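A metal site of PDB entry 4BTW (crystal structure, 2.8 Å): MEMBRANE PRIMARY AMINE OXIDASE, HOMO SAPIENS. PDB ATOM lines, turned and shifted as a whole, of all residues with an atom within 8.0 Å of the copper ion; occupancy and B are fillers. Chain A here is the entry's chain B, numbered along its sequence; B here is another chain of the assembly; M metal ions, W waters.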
ATOM      1  N   ALA A 344      -6.680  20.099  23.199  1.00  0.00           N
ATOM      2  CA  ALA A 344      -5.963  19.868  24.450  1.00  0.00           C
ATOM      3  C   ALA A 344      -6.900  19.213  25.436  1.00  0.00           C
ATOM      4  O   ALA A 344      -7.959  19.772  25.705  1.00  0.00           O
ATOM      5  CB  ALA A 344      -5.487  21.199  25.025  1.00  0.00           C
ATOM      6  N   TYR A 346      -7.379  17.272  29.134  1.00  0.00           N
ATOM      7  CA  TYR A 346      -6.792  17.069  30.481  1.00  0.00           C
ATOM      8  C   TYR A 346      -7.217  15.852  31.341  1.00  0.00           C
ATOM      9  O   TYR A 346      -8.229  15.193  31.107  1.00  0.00           O
ATOM     10  CB  TYR A 346      -6.967  18.326  31.292  1.00  0.00           C
ATOM     11  CG  TYR A 346      -6.081  19.421  30.786  1.00  0.00           C
ATOM     12  CD1 TYR A 346      -4.783  19.570  31.236  1.00  0.00           C
ATOM     13  CD2 TYR A 346      -6.527  20.299  29.808  1.00  0.00           C
ATOM     14  CE1 TYR A 346      -3.954  20.576  30.726  1.00  0.00           C
ATOM     15  CE2 TYR A 346      -5.713  21.326  29.314  1.00  0.00           C
ATOM     16  CZ  TYR A 346      -4.418  21.463  29.757  1.00  0.00           C
ATOM     17  OH  TYR A 346      -3.616  22.477  29.262  1.00  0.00           O
ATOM     18  N   ASN A 444      -2.547  29.675  28.552  1.00  0.00           N
ATOM     19  CA  ASN A 444      -1.273  29.360  29.063  1.00  0.00           C
ATOM     20  C   ASN A 444      -0.357  29.056  27.880  1.00  0.00           C
ATOM     21  O   ASN A 444       0.842  29.345  27.916  1.00  0.00           O
ATOM     22  CB  ASN A 444      -1.385  28.205  30.052  1.00  0.00           C
ATOM     23  CG  ASN A 444      -1.965  26.973  29.411  1.00  0.00           C
ATOM     24  OD1 ASN A 444      -1.230  26.116  28.941  1.00  0.00           O
ATOM     25  ND2 ASN A 444      -3.292  26.870  29.374  1.00  0.00           N
ATOM     26  N   TPQ A 445      -0.935  28.553  26.783  1.00  0.00           N
ATOM     27  CA  TPQ A 445      -0.107  28.064  25.672  1.00  0.00           C
ATOM     28  CB  TPQ A 445      -0.767  27.030  24.784  1.00  0.00           C
ATOM     29  C   TPQ A 445       0.303  29.143  24.721  1.00  0.00           C
ATOM     30  O   TPQ A 445      -0.479  30.045  24.361  1.00  0.00           O
ATOM     31  C1  TPQ A 445      -1.856  26.235  25.440  1.00  0.00           C
ATOM     32  C2  TPQ A 445      -1.492  24.927  26.066  1.00  0.00           C
ATOM     33  O2  TPQ A 445      -0.305  24.506  26.069  1.00  0.00           O
ATOM     34  C3  TPQ A 445      -2.522  24.181  26.651  1.00  0.00           C
ATOM     35  C4  TPQ A 445      -3.842  24.641  26.625  1.00  0.00           C
ATOM     36  O4  TPQ A 445      -4.762  23.849  27.213  1.00  0.00           O
ATOM     37  C5  TPQ A 445      -4.250  25.961  25.987  1.00  0.00           C
ATOM     38  O5  TPQ A 445      -5.462  26.386  25.963  1.00  0.00           O
ATOM     39  C6  TPQ A 445      -3.182  26.693  25.406  1.00  0.00           C
ATOM     40  N   TYR A 447       1.440  28.558  20.994  1.00  0.00           N
ATOM     41  CA  TYR A 447       1.482  27.562  19.930  1.00  0.00           C
ATOM     42  C   TYR A 447       2.360  28.143  18.843  1.00  0.00           C
ATOM     43  O   TYR A 447       2.217  29.324  18.469  1.00  0.00           O
ATOM     44  CB  TYR A 447       0.054  27.315  19.415  1.00  0.00           C
ATOM     45  CG  TYR A 447      -0.779  26.321  20.223  1.00  0.00           C
ATOM     46  CD1 TYR A 447      -0.317  25.029  20.439  1.00  0.00           C
ATOM     47  CD2 TYR A 447      -2.042  26.647  20.754  1.00  0.00           C
ATOM     48  CE1 TYR A 447      -1.045  24.079  21.173  1.00  0.00           C
ATOM     49  CE2 TYR A 447      -2.796  25.683  21.483  1.00  0.00           C
ATOM     50  CZ  TYR A 447      -2.280  24.386  21.691  1.00  0.00           C
ATOM     51  OH  TYR A 447      -2.921  23.349  22.368  1.00  0.00           O
ATOM     52  N   ALA A 465       4.379  23.366  20.920  1.00  0.00           N
ATOM     53  CA  ALA A 465       3.738  23.807  22.155  1.00  0.00           C
ATOM     54  C   ALA A 465       4.796  24.317  23.135  1.00  0.00           C
ATOM     55  O   ALA A 465       5.638  23.524  23.637  1.00  0.00           O
ATOM     56  CB  ALA A 465       2.992  22.644  22.769  1.00  0.00           C
ATOM     57  N   THR A 466       4.768  25.629  23.354  1.00  0.00           N
ATOM     58  CA  THR A 466       5.595  26.287  24.370  1.00  0.00           C
ATOM     59  C   THR A 466       4.672  27.266  25.153  1.00  0.00           C
ATOM     60  O   THR A 466       3.467  27.162  25.066  1.00  0.00           O
ATOM     61  CB  THR A 466       6.845  26.977  23.758  1.00  0.00           C
ATOM     62  OG1 THR A 466       7.742  27.344  24.810  1.00  0.00           O
ATOM     63  CG2 THR A 466       6.485  28.230  22.964  1.00  0.00           C
ATOM     64  N   GLY A 467       5.233  28.214  25.895  1.00  0.00           N
ATOM     65  CA  GLY A 467       4.448  28.971  26.847  1.00  0.00           C
ATOM     66  C   GLY A 467       4.312  28.231  28.186  1.00  0.00           C
ATOM     67  O   GLY A 467       5.044  27.259  28.462  1.00  0.00           O
ATOM     68  N   TYR A 468       3.371  28.702  29.000  1.00  0.00           N
ATOM     69  CA  TYR A 468       3.122  28.151  30.342  1.00  0.00           C
ATOM     70  C   TYR A 468       2.257  26.904  30.284  1.00  0.00           C
ATOM     71  O   TYR A 468       1.579  26.702  29.311  1.00  0.00           O
ATOM     72  CB  TYR A 468       2.427  29.197  31.232  1.00  0.00           C
ATOM     73  CG  TYR A 468       3.368  30.166  31.904  1.00  0.00           C
ATOM     74  CD1 TYR A 468       3.962  29.842  33.120  1.00  0.00           C
ATOM     75  CD2 TYR A 468       3.664  31.435  31.314  1.00  0.00           C
ATOM     76  CE1 TYR A 468       4.812  30.729  33.735  1.00  0.00           C
ATOM     77  CE2 TYR A 468       4.528  32.324  31.932  1.00  0.00           C
ATOM     78  CZ  TYR A 468       5.104  31.959  33.156  1.00  0.00           C
ATOM     79  OH  TYR A 468       5.966  32.807  33.844  1.00  0.00           O
ATOM     80  N   ILE A 469       2.290  26.105  31.342  1.00  0.00           N
ATOM     81  CA  ILE A 469       1.310  25.019  31.508  1.00  0.00           C
ATOM     82  C   ILE A 469       0.064  25.456  32.302  1.00  0.00           C
ATOM     83  O   ILE A 469       0.020  26.554  32.878  1.00  0.00           O
ATOM     84  CB  ILE A 469       1.935  23.794  32.182  1.00  0.00           C
ATOM     85  CG1 ILE A 469       2.315  24.059  33.645  1.00  0.00           C
ATOM     86  CG2 ILE A 469       3.174  23.383  31.434  1.00  0.00           C
ATOM     87  CD1 ILE A 469       2.741  22.792  34.354  1.00  0.00           C
ATOM     88  N   SER A 470      -0.955  24.583  32.289  1.00  0.00           N
ATOM     89  CA  SER A 470      -2.119  24.736  33.157  1.00  0.00           C
ATOM     90  C   SER A 470      -1.763  23.956  34.395  1.00  0.00           C
ATOM     91  O   SER A 470      -1.256  22.827  34.295  1.00  0.00           O
ATOM     92  CB  SER A 470      -3.386  24.149  32.537  1.00  0.00           C
ATOM     93  OG  SER A 470      -3.689  24.729  31.276  1.00  0.00           O
ATOM     94  N   THR A 492      -0.593  19.247  35.280  1.00  0.00           N
ATOM     95  CA  THR A 492      -1.807  18.510  35.057  1.00  0.00           C
ATOM     96  C   THR A 492      -1.711  17.805  33.702  1.00  0.00           C
ATOM     97  O   THR A 492      -1.421  18.442  32.698  1.00  0.00           O
ATOM     98  CB  THR A 492      -2.983  19.480  35.243  1.00  0.00           C
ATOM     99  OG1 THR A 492      -4.193  18.725  35.309  1.00  0.00           O
ATOM    100  CG2 THR A 492      -3.043  20.581  34.181  1.00  0.00           C
ATOM    101  N   VAL A 493      -1.872  16.480  33.709  1.00  0.00           N
ATOM    102  CA  VAL A 493      -1.531  15.691  32.534  1.00  0.00           C
ATOM    103  C   VAL A 493      -2.458  16.099  31.432  1.00  0.00           C
ATOM    104  O   VAL A 493      -3.620  16.367  31.686  1.00  0.00           O
ATOM    105  CB  VAL A 493      -1.632  14.150  32.756  1.00  0.00           C
ATOM    106  CG1 VAL A 493      -3.041  13.703  33.016  1.00  0.00           C
ATOM    107  CG2 VAL A 493      -1.175  13.382  31.542  1.00  0.00           C
ATOM    108  N   HIS A 494      -1.952  16.151  30.202  1.00  0.00           N
ATOM    109  CA  HIS A 494      -2.846  16.322  29.062  1.00  0.00           C
ATOM    110  C   HIS A 494      -2.268  15.745  27.789  1.00  0.00           C
ATOM    111  O   HIS A 494      -1.147  15.234  27.794  1.00  0.00           O
ATOM    112  CB  HIS A 494      -3.119  17.785  28.859  1.00  0.00           C
ATOM    113  CG  HIS A 494      -1.884  18.579  28.758  1.00  0.00           C
ATOM    114  ND1 HIS A 494      -1.251  19.082  29.869  1.00  0.00           N
ATOM    115  CD2 HIS A 494      -1.102  18.888  27.708  1.00  0.00           C
ATOM    116  CE1 HIS A 494      -0.162  19.723  29.486  1.00  0.00           C
ATOM    117  NE2 HIS A 494      -0.048  19.620  28.185  1.00  0.00           N
ATOM    118  N   THR A 495      -3.082  15.795  26.711  1.00  0.00           N
ATOM    119  CA  THR A 495      -2.616  15.517  25.355  1.00  0.00           C
ATOM    120  C   THR A 495      -2.740  16.815  24.585  1.00  0.00           C
ATOM    121  O   THR A 495      -3.571  17.634  24.954  1.00  0.00           O
ATOM    122  CB  THR A 495      -3.411  14.388  24.642  1.00  0.00           C
ATOM    123  OG1 THR A 495      -4.780  14.770  24.401  1.00  0.00           O
ATOM    124  CG2 THR A 495      -3.396  13.134  25.469  1.00  0.00           C
ATOM    125  N   HIS A 496      -1.861  17.043  23.589  1.00  0.00           N
ATOM    126  CA  HIS A 496      -2.145  17.987  22.497  1.00  0.00           C
ATOM    127  C   HIS A 496      -2.364  17.243  21.164  1.00  0.00           C
ATOM    128  O   HIS A 496      -1.872  16.095  20.946  1.00  0.00           O
ATOM    129  CB  HIS A 496      -1.032  18.989  22.256  1.00  0.00           C
ATOM    130  CG  HIS A 496      -0.588  19.726  23.476  1.00  0.00           C
ATOM    131  ND1 HIS A 496      -0.982  21.025  23.730  1.00  0.00           N
ATOM    132  CD2 HIS A 496       0.272  19.376  24.475  1.00  0.00           C
ATOM    133  CE1 HIS A 496      -0.401  21.440  24.845  1.00  0.00           C
ATOM    134  NE2 HIS A 496       0.361  20.459  25.319  1.00  0.00           N
ATOM    135  N   PHE A 656       1.008  14.924  20.814  1.00  0.00           N
ATOM    136  CA  PHE A 656       1.759  14.136  21.777  1.00  0.00           C
ATOM    137  C   PHE A 656       1.063  14.118  23.138  1.00  0.00           C
ATOM    138  O   PHE A 656       0.142  14.937  23.383  1.00  0.00           O
ATOM    139  CB  PHE A 656       3.177  14.707  21.937  1.00  0.00           C
ATOM    140  CG  PHE A 656       3.202  16.171  22.232  1.00  0.00           C
ATOM    141  CD1 PHE A 656       3.099  17.100  21.223  1.00  0.00           C
ATOM    142  CD2 PHE A 656       3.356  16.623  23.516  1.00  0.00           C
ATOM    143  CE1 PHE A 656       3.136  18.467  21.474  1.00  0.00           C
ATOM    144  CE2 PHE A 656       3.373  17.981  23.792  1.00  0.00           C
ATOM    145  CZ  PHE A 656       3.256  18.918  22.778  1.00  0.00           C
ATOM    146  N   LEU A 657       1.495  13.167  23.975  1.00  0.00           N
ATOM    147  CA  LEU A 657       1.184  13.161  25.408  1.00  0.00           C
ATOM    148  C   LEU A 657       2.069  14.130  26.198  1.00  0.00           C
ATOM    149  O   LEU A 657       3.276  14.185  26.021  1.00  0.00           O
ATOM    150  CB  LEU A 657       1.366  11.768  25.961  1.00  0.00           C
ATOM    151  CG  LEU A 657       1.300  11.657  27.496  1.00  0.00           C
ATOM    152  CD1 LEU A 657       0.185  12.486  28.132  1.00  0.00           C
ATOM    153  CD2 LEU A 657       1.118  10.186  27.859  1.00  0.00           C
ATOM    154  N   HIS A 658       1.491  14.898  27.105  1.00  0.00           N
ATOM    155  CA  HIS A 658       2.299  15.814  27.882  1.00  0.00           C
ATOM    156  C   HIS A 658       2.060  15.684  29.383  1.00  0.00           C
ATOM    157  O   HIS A 658       1.017  16.147  29.880  1.00  0.00           O
ATOM    158  CB  HIS A 658       1.980  17.229  27.468  1.00  0.00           C
ATOM    159  CG  HIS A 658       2.840  18.216  28.125  1.00  0.00           C
ATOM    160  ND1 HIS A 658       2.836  19.541  27.777  1.00  0.00           N
ATOM    161  CD2 HIS A 658       3.793  18.076  29.079  1.00  0.00           C
ATOM    162  CE1 HIS A 658       3.700  20.206  28.530  1.00  0.00           C
ATOM    163  NE2 HIS A 658       4.308  19.331  29.314  1.00  0.00           N
ATOM    164  N   ILE A 659       3.008  15.079  30.088  1.00  0.00           N
ATOM    165  CA  ILE A 659       2.954  14.876  31.541  1.00  0.00           C
ATOM    166  C   ILE A 659       3.825  15.926  32.202  1.00  0.00           C
ATOM    167  O   ILE A 659       5.031  15.704  32.363  1.00  0.00           O
ATOM    168  CB  ILE A 659       3.532  13.487  31.899  1.00  0.00           C
ATOM    169  CG1 ILE A 659       2.749  12.393  31.207  1.00  0.00           C
ATOM    170  CG2 ILE A 659       3.494  13.221  33.392  1.00  0.00           C
ATOM    171  CD1 ILE A 659       3.147  10.980  31.633  1.00  0.00           C
ATOM    172  N   PRO A 660       3.276  17.064  32.612  1.00  0.00           N
ATOM    173  CA  PRO A 660       4.306  18.084  32.919  1.00  0.00           C
ATOM    174  C   PRO A 660       5.289  17.703  34.018  1.00  0.00           C
ATOM    175  O   PRO A 660       4.975  16.892  34.896  1.00  0.00           O
ATOM    176  CB  PRO A 660       3.495  19.349  33.258  1.00  0.00           C
ATOM    177  CG  PRO A 660       2.186  19.135  32.579  1.00  0.00           C
ATOM    178  CD  PRO A 660       1.922  17.637  32.617  1.00  0.00           C
ATOM    179  N   ASP A 664       9.386  22.265  32.990  1.00  0.00           N
ATOM    180  CA  ASP A 664       8.372  23.032  32.265  1.00  0.00           C
ATOM    181  C   ASP A 664       8.130  24.364  32.956  1.00  0.00           C
ATOM    182  O   ASP A 664       7.279  25.146  32.533  1.00  0.00           O
ATOM    183  CB  ASP A 664       7.062  22.237  32.149  1.00  0.00           C
ATOM    184  CG  ASP A 664       7.138  21.081  31.148  1.00  0.00           C
ATOM    185  OD1 ASP A 664       7.829  21.198  30.125  1.00  0.00           O
ATOM    186  OD2 ASP A 664       6.518  20.033  31.384  1.00  0.00           O
ATOM    187  N   THR A 668       7.241  25.385  29.039  1.00  0.00           N
ATOM    188  CA  THR A 668       7.557  24.240  28.235  1.00  0.00           C
ATOM    189  C   THR A 668       8.442  24.741  27.078  1.00  0.00           C
ATOM    190  O   THR A 668       8.252  25.828  26.528  1.00  0.00           O
ATOM    191  CB  THR A 668       6.304  23.509  27.664  1.00  0.00           C
ATOM    192  OG1 THR A 668       5.099  23.780  28.399  1.00  0.00           O
ATOM    193  CG2 THR A 668       6.547  21.999  27.645  1.00  0.00           C
ATOM    194  N   ASN A 673       9.296  18.548  21.020  1.00  0.00           N
ATOM    195  CA  ASN A 673       7.855  18.772  20.954  1.00  0.00           C
ATOM    196  C   ASN A 673       7.426  19.384  19.607  1.00  0.00           C
ATOM    197  O   ASN A 673       6.402  20.109  19.507  1.00  0.00           O
ATOM    198  CB  ASN A 673       7.434  19.738  22.090  1.00  0.00           C
ATOM    199  CG  ASN A 673       7.334  19.057  23.453  1.00  0.00           C
ATOM    200  OD1 ASN A 673       7.579  17.846  23.592  1.00  0.00           O
ATOM    201  ND2 ASN A 673       6.947  19.837  24.479  1.00  0.00           N
ATOM    202  N   TYR B 560       6.346   7.758  27.700  1.00  0.00           N
ATOM    203  CA  TYR B 560       7.416   8.350  28.535  1.00  0.00           C
ATOM    204  C   TYR B 560       8.254   7.212  29.119  1.00  0.00           C
ATOM    205  O   TYR B 560       7.836   6.530  30.067  1.00  0.00           O
ATOM    206  CB  TYR B 560       6.881   9.190  29.685  1.00  0.00           C
ATOM    207  CG  TYR B 560       6.519  10.599  29.335  1.00  0.00           C
ATOM    208  CD1 TYR B 560       5.484  10.866  28.485  1.00  0.00           C
ATOM    209  CD2 TYR B 560       7.188  11.669  29.899  1.00  0.00           C
ATOM    210  CE1 TYR B 560       5.129  12.170  28.177  1.00  0.00           C
ATOM    211  CE2 TYR B 560       6.852  12.977  29.603  1.00  0.00           C
ATOM    212  CZ  TYR B 560       5.832  13.223  28.737  1.00  0.00           C
ATOM    213  OH  TYR B 560       5.499  14.517  28.407  1.00  0.00           O
HETATM  214 CU    CU M   1       1.359  20.607  27.087  1.00  0.00          CU
HETATM  215  O   HOH W   1       1.353  22.506  27.458  1.00  0.00           O
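OD2 of Asp 664 lies within hydrogen-bond range of NE2 of His 658 (3.1 Å).
N of His 496 is in hydrogen-bond range of O of Phe 656 (2.9 Å).
The side-chain hydroxyl (OH) of Tyr 447 sits at hydrogen-bond distance from a ring nitrogen (ND1) of His 496, at 3.3 Å.
ND1 of His 494 is in hydrogen-bond range of O of Thr 492 (2.9 Å).
Of the 25 residues printed, 3 come within 4 Å of the copper ion.
The nearest printed residue that does not touch the copper ion is TPQ 445 (4.4 Å).
The copper ion is bound by water W1, a ring nitrogen (ND1) of His 658, a ring nitrogen (NE2) of His 496 and a ring nitrogen (NE2) of His 494.
The copper ion has four donor atoms within binding distance.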
